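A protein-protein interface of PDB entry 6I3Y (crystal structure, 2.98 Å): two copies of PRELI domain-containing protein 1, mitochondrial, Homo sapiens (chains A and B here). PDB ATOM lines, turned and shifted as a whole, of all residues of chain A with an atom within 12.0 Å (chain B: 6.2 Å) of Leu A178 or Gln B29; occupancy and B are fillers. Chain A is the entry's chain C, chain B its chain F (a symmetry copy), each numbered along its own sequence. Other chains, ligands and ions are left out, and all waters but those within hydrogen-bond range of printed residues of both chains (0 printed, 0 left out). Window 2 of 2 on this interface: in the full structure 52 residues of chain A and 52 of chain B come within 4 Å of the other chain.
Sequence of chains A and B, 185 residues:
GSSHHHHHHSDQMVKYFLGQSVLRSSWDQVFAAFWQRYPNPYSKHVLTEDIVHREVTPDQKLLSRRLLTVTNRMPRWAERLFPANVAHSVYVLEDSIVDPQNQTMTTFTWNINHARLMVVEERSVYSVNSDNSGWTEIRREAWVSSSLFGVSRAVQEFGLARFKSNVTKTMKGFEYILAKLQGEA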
ATOM      1  N   THR A 168      -2.469  35.030  11.176  1.00  0.00           N
ATOM      2  CA  THR A 168      -3.714  34.279  11.201  1.00  0.00           C
ATOM      3  C   THR A 168      -3.627  33.158  10.177  1.00  0.00           C
ATOM      4  O   THR A 168      -4.086  32.050  10.440  1.00  0.00           O
ATOM      5  CB  THR A 168      -4.926  35.158  10.867  1.00  0.00           C
ATOM      6  OG1 THR A 168      -4.772  35.705   9.554  1.00  0.00           O
ATOM      7  CG2 THR A 168      -5.071  36.285  11.851  1.00  0.00           C
ATOM      8  N   LYS A 169      -3.023  33.456   9.028  1.00  0.00           N
ATOM      9  CA  LYS A 169      -2.848  32.466   7.970  1.00  0.00           C
ATOM     10  C   LYS A 169      -2.000  31.285   8.429  1.00  0.00           C
ATOM     11  O   LYS A 169      -2.285  30.134   8.096  1.00  0.00           O
ATOM     12  CB  LYS A 169      -2.225  33.090   6.722  1.00  0.00           C
ATOM     13  CG  LYS A 169      -3.163  34.047   5.995  1.00  0.00           C
ATOM     14  CD  LYS A 169      -2.597  34.509   4.657  1.00  0.00           C
ATOM     15  N   THR A 170      -0.973  31.583   9.211  1.00  0.00           N
ATOM     16  CA  THR A 170      -0.116  30.546   9.733  1.00  0.00           C
ATOM     17  C   THR A 170      -0.889  29.554  10.628  1.00  0.00           C
ATOM     18  O   THR A 170      -0.702  28.355  10.555  1.00  0.00           O
ATOM     19  CB  THR A 170       1.076  31.119  10.500  1.00  0.00           C
ATOM     20  OG1 THR A 170       1.986  30.050  10.775  1.00  0.00           O
ATOM     21  CG2 THR A 170       0.674  31.794  11.784  1.00  0.00           C
ATOM     22  N   MET A 171      -1.768  30.084  11.458  1.00  0.00           N
ATOM     23  CA  MET A 171      -2.554  29.241  12.319  1.00  0.00           C
ATOM     24  C   MET A 171      -3.510  28.393  11.489  1.00  0.00           C
ATOM     25  O   MET A 171      -3.650  27.193  11.733  1.00  0.00           O
ATOM     26  CB  MET A 171      -3.308  30.073  13.360  1.00  0.00           C
ATOM     27  CG  MET A 171      -2.359  30.868  14.268  1.00  0.00           C
ATOM     28  SD  MET A 171      -0.892  29.956  14.834  1.00  0.00           S
ATOM     29  CE  MET A 171      -1.713  28.674  15.749  1.00  0.00           C
ATOM     30  N   LYS A 172      -4.150  29.012  10.503  1.00  0.00           N
ATOM     31  CA  LYS A 172      -5.012  28.282   9.557  1.00  0.00           C
ATOM     32  C   LYS A 172      -4.219  27.156   8.874  1.00  0.00           C
ATOM     33  O   LYS A 172      -4.568  25.975   8.998  1.00  0.00           O
ATOM     34  CB  LYS A 172      -5.642  29.227   8.503  1.00  0.00           C
ATOM     35  CG  LYS A 172      -7.097  29.631   8.740  1.00  0.00           C
ATOM     36  CD  LYS A 172      -7.270  30.602   9.894  1.00  0.00           C
ATOM     37  N   GLY A 173      -3.147  27.526   8.183  1.00  0.00           N
ATOM     38  CA  GLY A 173      -2.268  26.559   7.539  1.00  0.00           C
ATOM     39  C   GLY A 173      -1.623  25.563   8.489  1.00  0.00           C
ATOM     40  O   GLY A 173      -1.298  24.445   8.108  1.00  0.00           O
ATOM     41  N   PHE A 174      -1.431  25.962   9.736  1.00  0.00           N
ATOM     42  CA  PHE A 174      -0.871  25.054  10.723  1.00  0.00           C
ATOM     43  C   PHE A 174      -1.901  24.048  11.186  1.00  0.00           C
ATOM     44  O   PHE A 174      -1.604  22.870  11.246  1.00  0.00           O
ATOM     45  CB  PHE A 174      -0.353  25.785  11.962  1.00  0.00           C
ATOM     46  CG  PHE A 174       0.990  25.326  12.409  1.00  0.00           C
ATOM     47  CD1 PHE A 174       1.317  23.970  12.421  1.00  0.00           C
ATOM     48  CD2 PHE A 174       1.947  26.250  12.825  1.00  0.00           C
ATOM     49  CE1 PHE A 174       2.576  23.547  12.832  1.00  0.00           C
ATOM     50  CE2 PHE A 174       3.202  25.830  13.238  1.00  0.00           C
ATOM     51  CZ  PHE A 174       3.515  24.477  13.243  1.00  0.00           C
ATOM     52  N   GLU A 175      -3.097  24.527  11.549  1.00  0.00           N
ATOM     53  CA  GLU A 175      -4.227  23.653  11.941  1.00  0.00           C
ATOM     54  C   GLU A 175      -4.582  22.673  10.809  1.00  0.00           C
ATOM     55  O   GLU A 175      -4.690  21.472  11.038  1.00  0.00           O
ATOM     56  CB  GLU A 175      -5.449  24.480  12.388  1.00  0.00           C
ATOM     57  N   TYR A 176      -4.703  23.196   9.591  1.00  0.00           N
ATOM     58  CA  TYR A 176      -4.960  22.385   8.404  1.00  0.00           C
ATOM     59  C   TYR A 176      -3.994  21.240   8.286  1.00  0.00           C
ATOM     60  O   TYR A 176      -4.445  20.119   8.238  1.00  0.00           O
ATOM     61  CB  TYR A 176      -4.915  23.233   7.121  1.00  0.00           C
ATOM     62  CG  TYR A 176      -4.887  22.475   5.789  1.00  0.00           C
ATOM     63  CD1 TYR A 176      -3.723  21.819   5.360  1.00  0.00           C
ATOM     64  CD2 TYR A 176      -6.004  22.466   4.937  1.00  0.00           C
ATOM     65  CE1 TYR A 176      -3.668  21.157   4.149  1.00  0.00           C
ATOM     66  CE2 TYR A 176      -5.969  21.790   3.724  1.00  0.00           C
ATOM     67  CZ  TYR A 176      -4.802  21.147   3.329  1.00  0.00           C
ATOM     68  OH  TYR A 176      -4.770  20.490   2.123  1.00  0.00           O
ATOM     69  N   ILE A 177      -2.688  21.492   8.227  1.00  0.00           N
ATOM     70  CA  ILE A 177      -1.785  20.378   7.909  1.00  0.00           C
ATOM     71  C   ILE A 177      -1.658  19.463   9.119  1.00  0.00           C
ATOM     72  O   ILE A 177      -1.532  18.273   8.950  1.00  0.00           O
ATOM     73  CB  ILE A 177      -0.398  20.740   7.316  1.00  0.00           C
ATOM     74  CG1 ILE A 177       0.532  21.265   8.388  1.00  0.00           C
ATOM     75  CG2 ILE A 177      -0.471  21.662   6.106  1.00  0.00           C
ATOM     76  CD1 ILE A 177       1.476  20.183   8.838  1.00  0.00           C
ATOM     77  N   LEU A 178      -1.761  19.986  10.330  1.00  0.00           N
ATOM     78  CA  LEU A 178      -1.925  19.100  11.498  1.00  0.00           C
ATOM     79  C   LEU A 178      -3.053  18.087  11.331  1.00  0.00           C
ATOM     80  O   LEU A 178      -2.877  16.918  11.661  1.00  0.00           O
ATOM     81  CB  LEU A 178      -2.168  19.881  12.789  1.00  0.00           C
ATOM     82  CG  LEU A 178      -0.884  20.304  13.478  1.00  0.00           C
ATOM     83  CD1 LEU A 178      -1.174  21.343  14.547  1.00  0.00           C
ATOM     84  CD2 LEU A 178      -0.168  19.097  14.057  1.00  0.00           C
ATOM     85  N   ALA A 179      -4.205  18.536  10.835  1.00  0.00           N
ATOM     86  CA  ALA A 179      -5.317  17.629  10.554  1.00  0.00           C
ATOM     87  C   ALA A 179      -4.953  16.570   9.514  1.00  0.00           C
ATOM     88  O   ALA A 179      -5.366  15.417   9.647  1.00  0.00           O
ATOM     89  CB  ALA A 179      -6.549  18.399  10.116  1.00  0.00           C
ATOM     90  N   LYS A 180      -4.166  16.952   8.506  1.00  0.00           N
ATOM     91  CA  LYS A 180      -3.770  16.031   7.452  1.00  0.00           C
ATOM     92  C   LYS A 180      -2.801  14.937   7.904  1.00  0.00           C
ATOM     93  O   LYS A 180      -2.682  13.938   7.208  1.00  0.00           O
ATOM     94  CB  LYS A 180      -3.214  16.794   6.222  1.00  0.00           C
ATOM     95  CG  LYS A 180      -3.472  16.169   4.854  1.00  0.00           C
ATOM     96  CD  LYS A 180      -4.779  15.380   4.761  1.00  0.00           C
ATOM     97  CE  LYS A 180      -5.171  14.999   3.325  1.00  0.00           C
ATOM     98  NZ  LYS A 180      -6.262  15.879   2.849  1.00  0.00           N
ATOM     99  N   LEU A 181      -2.151  15.105   9.054  1.00  0.00           N
ATOM    100  CA  LEU A 181      -1.241  14.138   9.556  1.00  0.00           C
ATOM    101  C   LEU A 181      -1.873  13.108  10.451  1.00  0.00           C
ATOM    102  O   LEU A 181      -1.424  11.953  10.480  1.00  0.00           O
ATOM    103  CB  LEU A 181      -0.108  14.837  10.302  1.00  0.00           C
ATOM    104  CG  LEU A 181       1.230  14.667   9.617  1.00  0.00           C
ATOM    105  CD1 LEU A 181       1.374  13.195   9.244  1.00  0.00           C
ATOM    106  CD2 LEU A 181       1.373  15.582   8.408  1.00  0.00           C
ATOM    107  N   GLN A 182      -2.913  13.514  11.176  1.00  0.00           N
ATOM    108  CA  GLN A 182      -3.603  12.588  12.058  1.00  0.00           C
ATOM    109  C   GLN A 182      -4.206  11.482  11.211  1.00  0.00           C
ATOM    110  O   GLN A 182      -4.837  11.764  10.188  1.00  0.00           O
ATOM    111  CB  GLN A 182      -4.696  13.280  12.858  1.00  0.00           C
ATOM    112  N   GLY A 183      -3.927  10.237  11.592  1.00  0.00           N
ATOM    113  CA  GLY A 183      -4.458   9.060  10.909  1.00  0.00           C
ATOM    114  C   GLY A 183      -4.178   9.048   9.414  1.00  0.00           C
ATOM    115  O   GLY A 183      -5.066   8.731   8.620  1.00  0.00           O
ATOM    116  N   GLU A 184      -2.956   9.422   9.035  1.00  0.00           N
ATOM    117  CA  GLU A 184      -2.535   9.459   7.625  1.00  0.00           C
ATOM    118  C   GLU A 184      -3.508  10.205   6.699  1.00  0.00           C
ATOM    119  O   GLU A 184      -4.068  11.243   7.059  1.00  0.00           O
ATOM    120  CB  GLU A 184      -2.316   8.036   7.100  1.00  0.00           C
ATOM    121  N   LEU B  23      -2.376  25.498  19.820  1.00  0.00           N
ATOM    122  CA  LEU B  23      -2.833  24.519  18.844  1.00  0.00           C
ATOM    123  C   LEU B  23      -3.344  23.281  19.569  1.00  0.00           C
ATOM    124  O   LEU B  23      -2.712  22.799  20.523  1.00  0.00           O
ATOM    125  CB  LEU B  23      -1.718  24.138  17.869  1.00  0.00           C
ATOM    126  CG  LEU B  23      -1.421  25.134  16.754  1.00  0.00           C
ATOM    127  CD1 LEU B  23      -0.339  24.599  15.815  1.00  0.00           C
ATOM    128  CD2 LEU B  23      -2.702  25.476  15.996  1.00  0.00           C
ATOM    129  N   ARG B  24      -4.447  22.757  19.034  1.00  0.00           N
ATOM    130  CA  ARG B  24      -5.114  21.677  19.626  1.00  0.00           C
ATOM    131  C   ARG B  24      -4.469  20.316  19.173  1.00  0.00           C
ATOM    132  O   ARG B  24      -5.151  19.425  18.715  1.00  0.00           O
ATOM    133  CB  ARG B  24      -6.648  21.808  19.466  1.00  0.00           C
ATOM    134  N   SER B  25      -3.149  20.186  19.356  1.00  0.00           N
ATOM    135  CA  SER B  25      -2.368  18.995  18.989  1.00  0.00           C
ATOM    136  C   SER B  25      -1.234  18.846  19.973  1.00  0.00           C
ATOM    137  O   SER B  25      -0.942  19.784  20.694  1.00  0.00           O
ATOM    138  CB  SER B  25      -1.781  19.143  17.578  1.00  0.00           C
ATOM    139  OG  SER B  25      -2.793  19.368  16.589  1.00  0.00           O
ATOM    140  N   SER B  26      -0.586  17.688  19.994  1.00  0.00           N
ATOM    141  CA  SER B  26       0.554  17.444  20.899  1.00  0.00           C
ATOM    142  C   SER B  26       1.796  18.149  20.377  1.00  0.00           C
ATOM    143  O   SER B  26       1.868  18.481  19.189  1.00  0.00           O
ATOM    144  CB  SER B  26       0.831  15.949  21.031  1.00  0.00           C
ATOM    145  OG  SER B  26       1.180  15.401  19.768  1.00  0.00           O
ATOM    146  N   TRP B  27       2.767  18.383  21.255  1.00  0.00           N
ATOM    147  CA  TRP B  27       3.975  19.121  20.867  1.00  0.00           C
ATOM    148  C   TRP B  27       4.837  18.474  19.774  1.00  0.00           C
ATOM    149  O   TRP B  27       5.348  19.171  18.904  1.00  0.00           O
ATOM    150  CB  TRP B  27       4.834  19.463  22.097  1.00  0.00           C
ATOM    151  CG  TRP B  27       5.432  18.288  22.810  1.00  0.00           C
ATOM    152  CD1 TRP B  27       4.894  17.619  23.848  1.00  0.00           C
ATOM    153  CD2 TRP B  27       6.685  17.662  22.533  1.00  0.00           C
ATOM    154  NE1 TRP B  27       5.720  16.607  24.233  1.00  0.00           N
ATOM    155  CE2 TRP B  27       6.835  16.617  23.446  1.00  0.00           C
ATOM    156  CE3 TRP B  27       7.692  17.879  21.585  1.00  0.00           C
ATOM    157  CZ2 TRP B  27       7.955  15.785  23.454  1.00  0.00           C
ATOM    158  CZ3 TRP B  27       8.809  17.053  21.590  1.00  0.00           C
ATOM    159  CH2 TRP B  27       8.934  16.027  22.524  1.00  0.00           C
ATOM    160  N   ASP B  28       4.998  17.162  19.818  1.00  0.00           N
ATOM    161  CA  ASP B  28       5.833  16.468  18.840  1.00  0.00           C
ATOM    162  C   ASP B  28       5.292  16.626  17.430  1.00  0.00           C
ATOM    163  O   ASP B  28       6.058  16.842  16.489  1.00  0.00           O
ATOM    164  CB  ASP B  28       5.967  14.989  19.192  1.00  0.00           C
ATOM    165  CG  ASP B  28       4.648  14.359  19.575  1.00  0.00           C
ATOM    166  OD1 ASP B  28       3.686  15.117  19.834  1.00  0.00           O
ATOM    167  OD2 ASP B  28       4.572  13.120  19.622  1.00  0.00           O
ATOM    168  N   GLN B  29       3.976  16.558  17.295  1.00  0.00           N
ATOM    169  CA  GLN B  29       3.346  16.689  15.996  1.00  0.00           C
ATOM    170  C   GLN B  29       3.590  18.073  15.393  1.00  0.00           C
ATOM    171  O   GLN B  29       3.864  18.192  14.197  1.00  0.00           O
ATOM    172  CB  GLN B  29       1.847  16.429  16.097  1.00  0.00           C
ATOM    173  CG  GLN B  29       1.491  15.030  16.569  1.00  0.00           C
ATOM    174  CD  GLN B  29       0.002  14.748  16.486  1.00  0.00           C
ATOM    175  OE1 GLN B  29      -0.703  15.314  15.654  1.00  0.00           O
ATOM    176  NE2 GLN B  29      -0.480  13.850  17.333  1.00  0.00           N
ATOM    177  N   VAL B  30       3.507  19.111  16.225  1.00  0.00           N
ATOM    178  CA  VAL B  30       3.655  20.474  15.722  1.00  0.00           C
ATOM    179  C   VAL B  30       5.092  20.741  15.351  1.00  0.00           C
ATOM    180  O   VAL B  30       5.340  21.339  14.311  1.00  0.00           O
ATOM    181  CB  VAL B  30       3.087  21.546  16.663  1.00  0.00           C
ATOM    182  CG1 VAL B  30       1.670  21.157  17.058  1.00  0.00           C
ATOM    183  CG2 VAL B  30       3.968  21.748  17.874  1.00  0.00           C
ATOM    184  N   PHE B  31       6.035  20.225  16.139  1.00  0.00           N
ATOM    185  CA  PHE B  31       7.454  20.369  15.797  1.00  0.00           C
ATOM    186  C   PHE B  31       7.696  19.655  14.455  1.00  0.00           C
ATOM    187  O   PHE B  31       8.430  20.162  13.606  1.00  0.00           O
ATOM    188  CB  PHE B  31       8.407  19.786  16.855  1.00  0.00           C
ATOM    189  CG  PHE B  31       8.440  20.519  18.181  1.00  0.00           C
ATOM    190  CD1 PHE B  31       7.358  21.258  18.663  1.00  0.00           C
ATOM    191  CD2 PHE B  31       9.573  20.399  18.996  1.00  0.00           C
ATOM    192  CE1 PHE B  31       7.395  21.863  19.914  1.00  0.00           C
ATOM    193  CE2 PHE B  31       9.624  21.001  20.254  1.00  0.00           C
ATOM    194  CZ  PHE B  31       8.528  21.736  20.717  1.00  0.00           C
ATOM    195  N   ALA B  32       7.082  18.484  14.274  1.00  0.00           N
ATOM    196  CA  ALA B  32       7.234  17.713  13.032  1.00  0.00           C
ATOM    197  C   ALA B  32       6.477  18.322  11.857  1.00  0.00           C
ATOM    198  O   ALA B  32       6.876  18.149  10.699  1.00  0.00           O
ATOM    199  CB  ALA B  32       6.789  16.277  13.244  1.00  0.00           C
ATOM    200  N   ALA B  33       5.384  19.006  12.179  1.00  0.00           N
ATOM    201  CA  ALA B  33       4.535  19.684  11.207  1.00  0.00           C
ATOM    202  C   ALA B  33       5.070  21.052  10.829  1.00  0.00           C
ATOM    203  O   ALA B  33       4.695  21.597   9.797  1.00  0.00           O
ATOM    204  CB  ALA B  33       3.133  19.833  11.770  1.00  0.00           C
ATOM    205  N   PHE B  34       5.933  21.607  11.669  1.00  0.00           N
ATOM    206  CA  PHE B  34       6.585  22.892  11.387  1.00  0.00           C
ATOM    207  C   PHE B  34       7.503  22.880  10.141  1.00  0.00           C
ATOM    208  O   PHE B  34       7.733  23.911   9.531  1.00  0.00           O
ATOM    209  CB  PHE B  34       7.353  23.344  12.627  1.00  0.00           C
ATOM    210  CG  PHE B  34       8.212  24.539  12.421  1.00  0.00           C
ATOM    211  CD1 PHE B  34       7.692  25.810  12.577  1.00  0.00           C
ATOM    212  CD2 PHE B  34       9.560  24.386  12.096  1.00  0.00           C
ATOM    213  CE1 PHE B  34       8.504  26.918  12.410  1.00  0.00           C
ATOM    214  CE2 PHE B  34      10.379  25.490  11.912  1.00  0.00           C
ATOM    215  CZ  PHE B  34       9.850  26.759  12.070  1.00  0.00           C
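The side-chain hydroxyl (OG) of Ser B26 sits close to the side-chain amide nitrogen (NE2) of Gln B29.
Of chain B, only Leu B23, Ser B25, Gln B29 and Val B30 come within 4 Å of Leu A178. Gln B29 touches just one residue of chain A: Leu A178. Arg B24 touches none of the printed residues of chain A. Of chain A, only Leu A178 (3.3 Å) comes within 4 Å of Ser B25. No residue of chain A comes within 4 Å of Trp B27. No residue of chain A comes within 4 Å of Asp B28. Printed residues of chain A within 4 Å of Val B30: Phe A174 (3.8 Å) and Leu A178 (3.8 Å). No residue of chain A comes within 4 Å of Phe B31. No residue of chain A comes within 4 Å of Ala B32. Of the printed residues of chain B, Met A171 touches Leu B23. Printed residues of chain B within 4 Å of Ile A177: Ala B33 (3.4 Å). Lys A180 touches none of the printed residues of chain B. Thr A168 touches none of the printed residues of chain B. The nearest residue of chain A that does not touch Gln B29 is Gln A182 (5.3 Å). The nearest printed residue of chain B that does not touch Phe A174 is Gln B29 (5.7 Å).
Hydrophobic or aromatic side chains of chain B that line the printed part of chain A: Leu B23, Val B30 and Ala B33. Hydrophobic or aromatic side chains of chain A that line the printed part of chain B: Met A171, Phe A174, Ile A177 and Leu A178. Among the printed residues, 10 pairs touch across the chains. Among the printed residues, no Asp or Glu carboxylate lies within 4 Å of a Lys or Arg side-chain nitrogen of the other chain.
No position is printed for both chains. Of the 10 pairs that touch across the chains among the printed residues, none has its exchanged pair printed and touching as well.
Among the printed residues, merely in contact across the chains: Met A171 with Leu B23 (3.4 Å), Phe A174 with Leu B23 (3.7 Å), Phe A174 with Val B30 (3.8 Å), Phe A174 with Ala B33 (3.9 Å), Phe A174 with Phe B34 (3.9 Å), Ile A177 with Ala B33 (3.4 Å), Leu A178 with Leu B23 (3.6 Å), Leu A178 with Ser B25 (3.3 Å), Leu A178 with Gln B29 (3.9 Å) and Leu A178 with Val B30 (3.8 Å).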
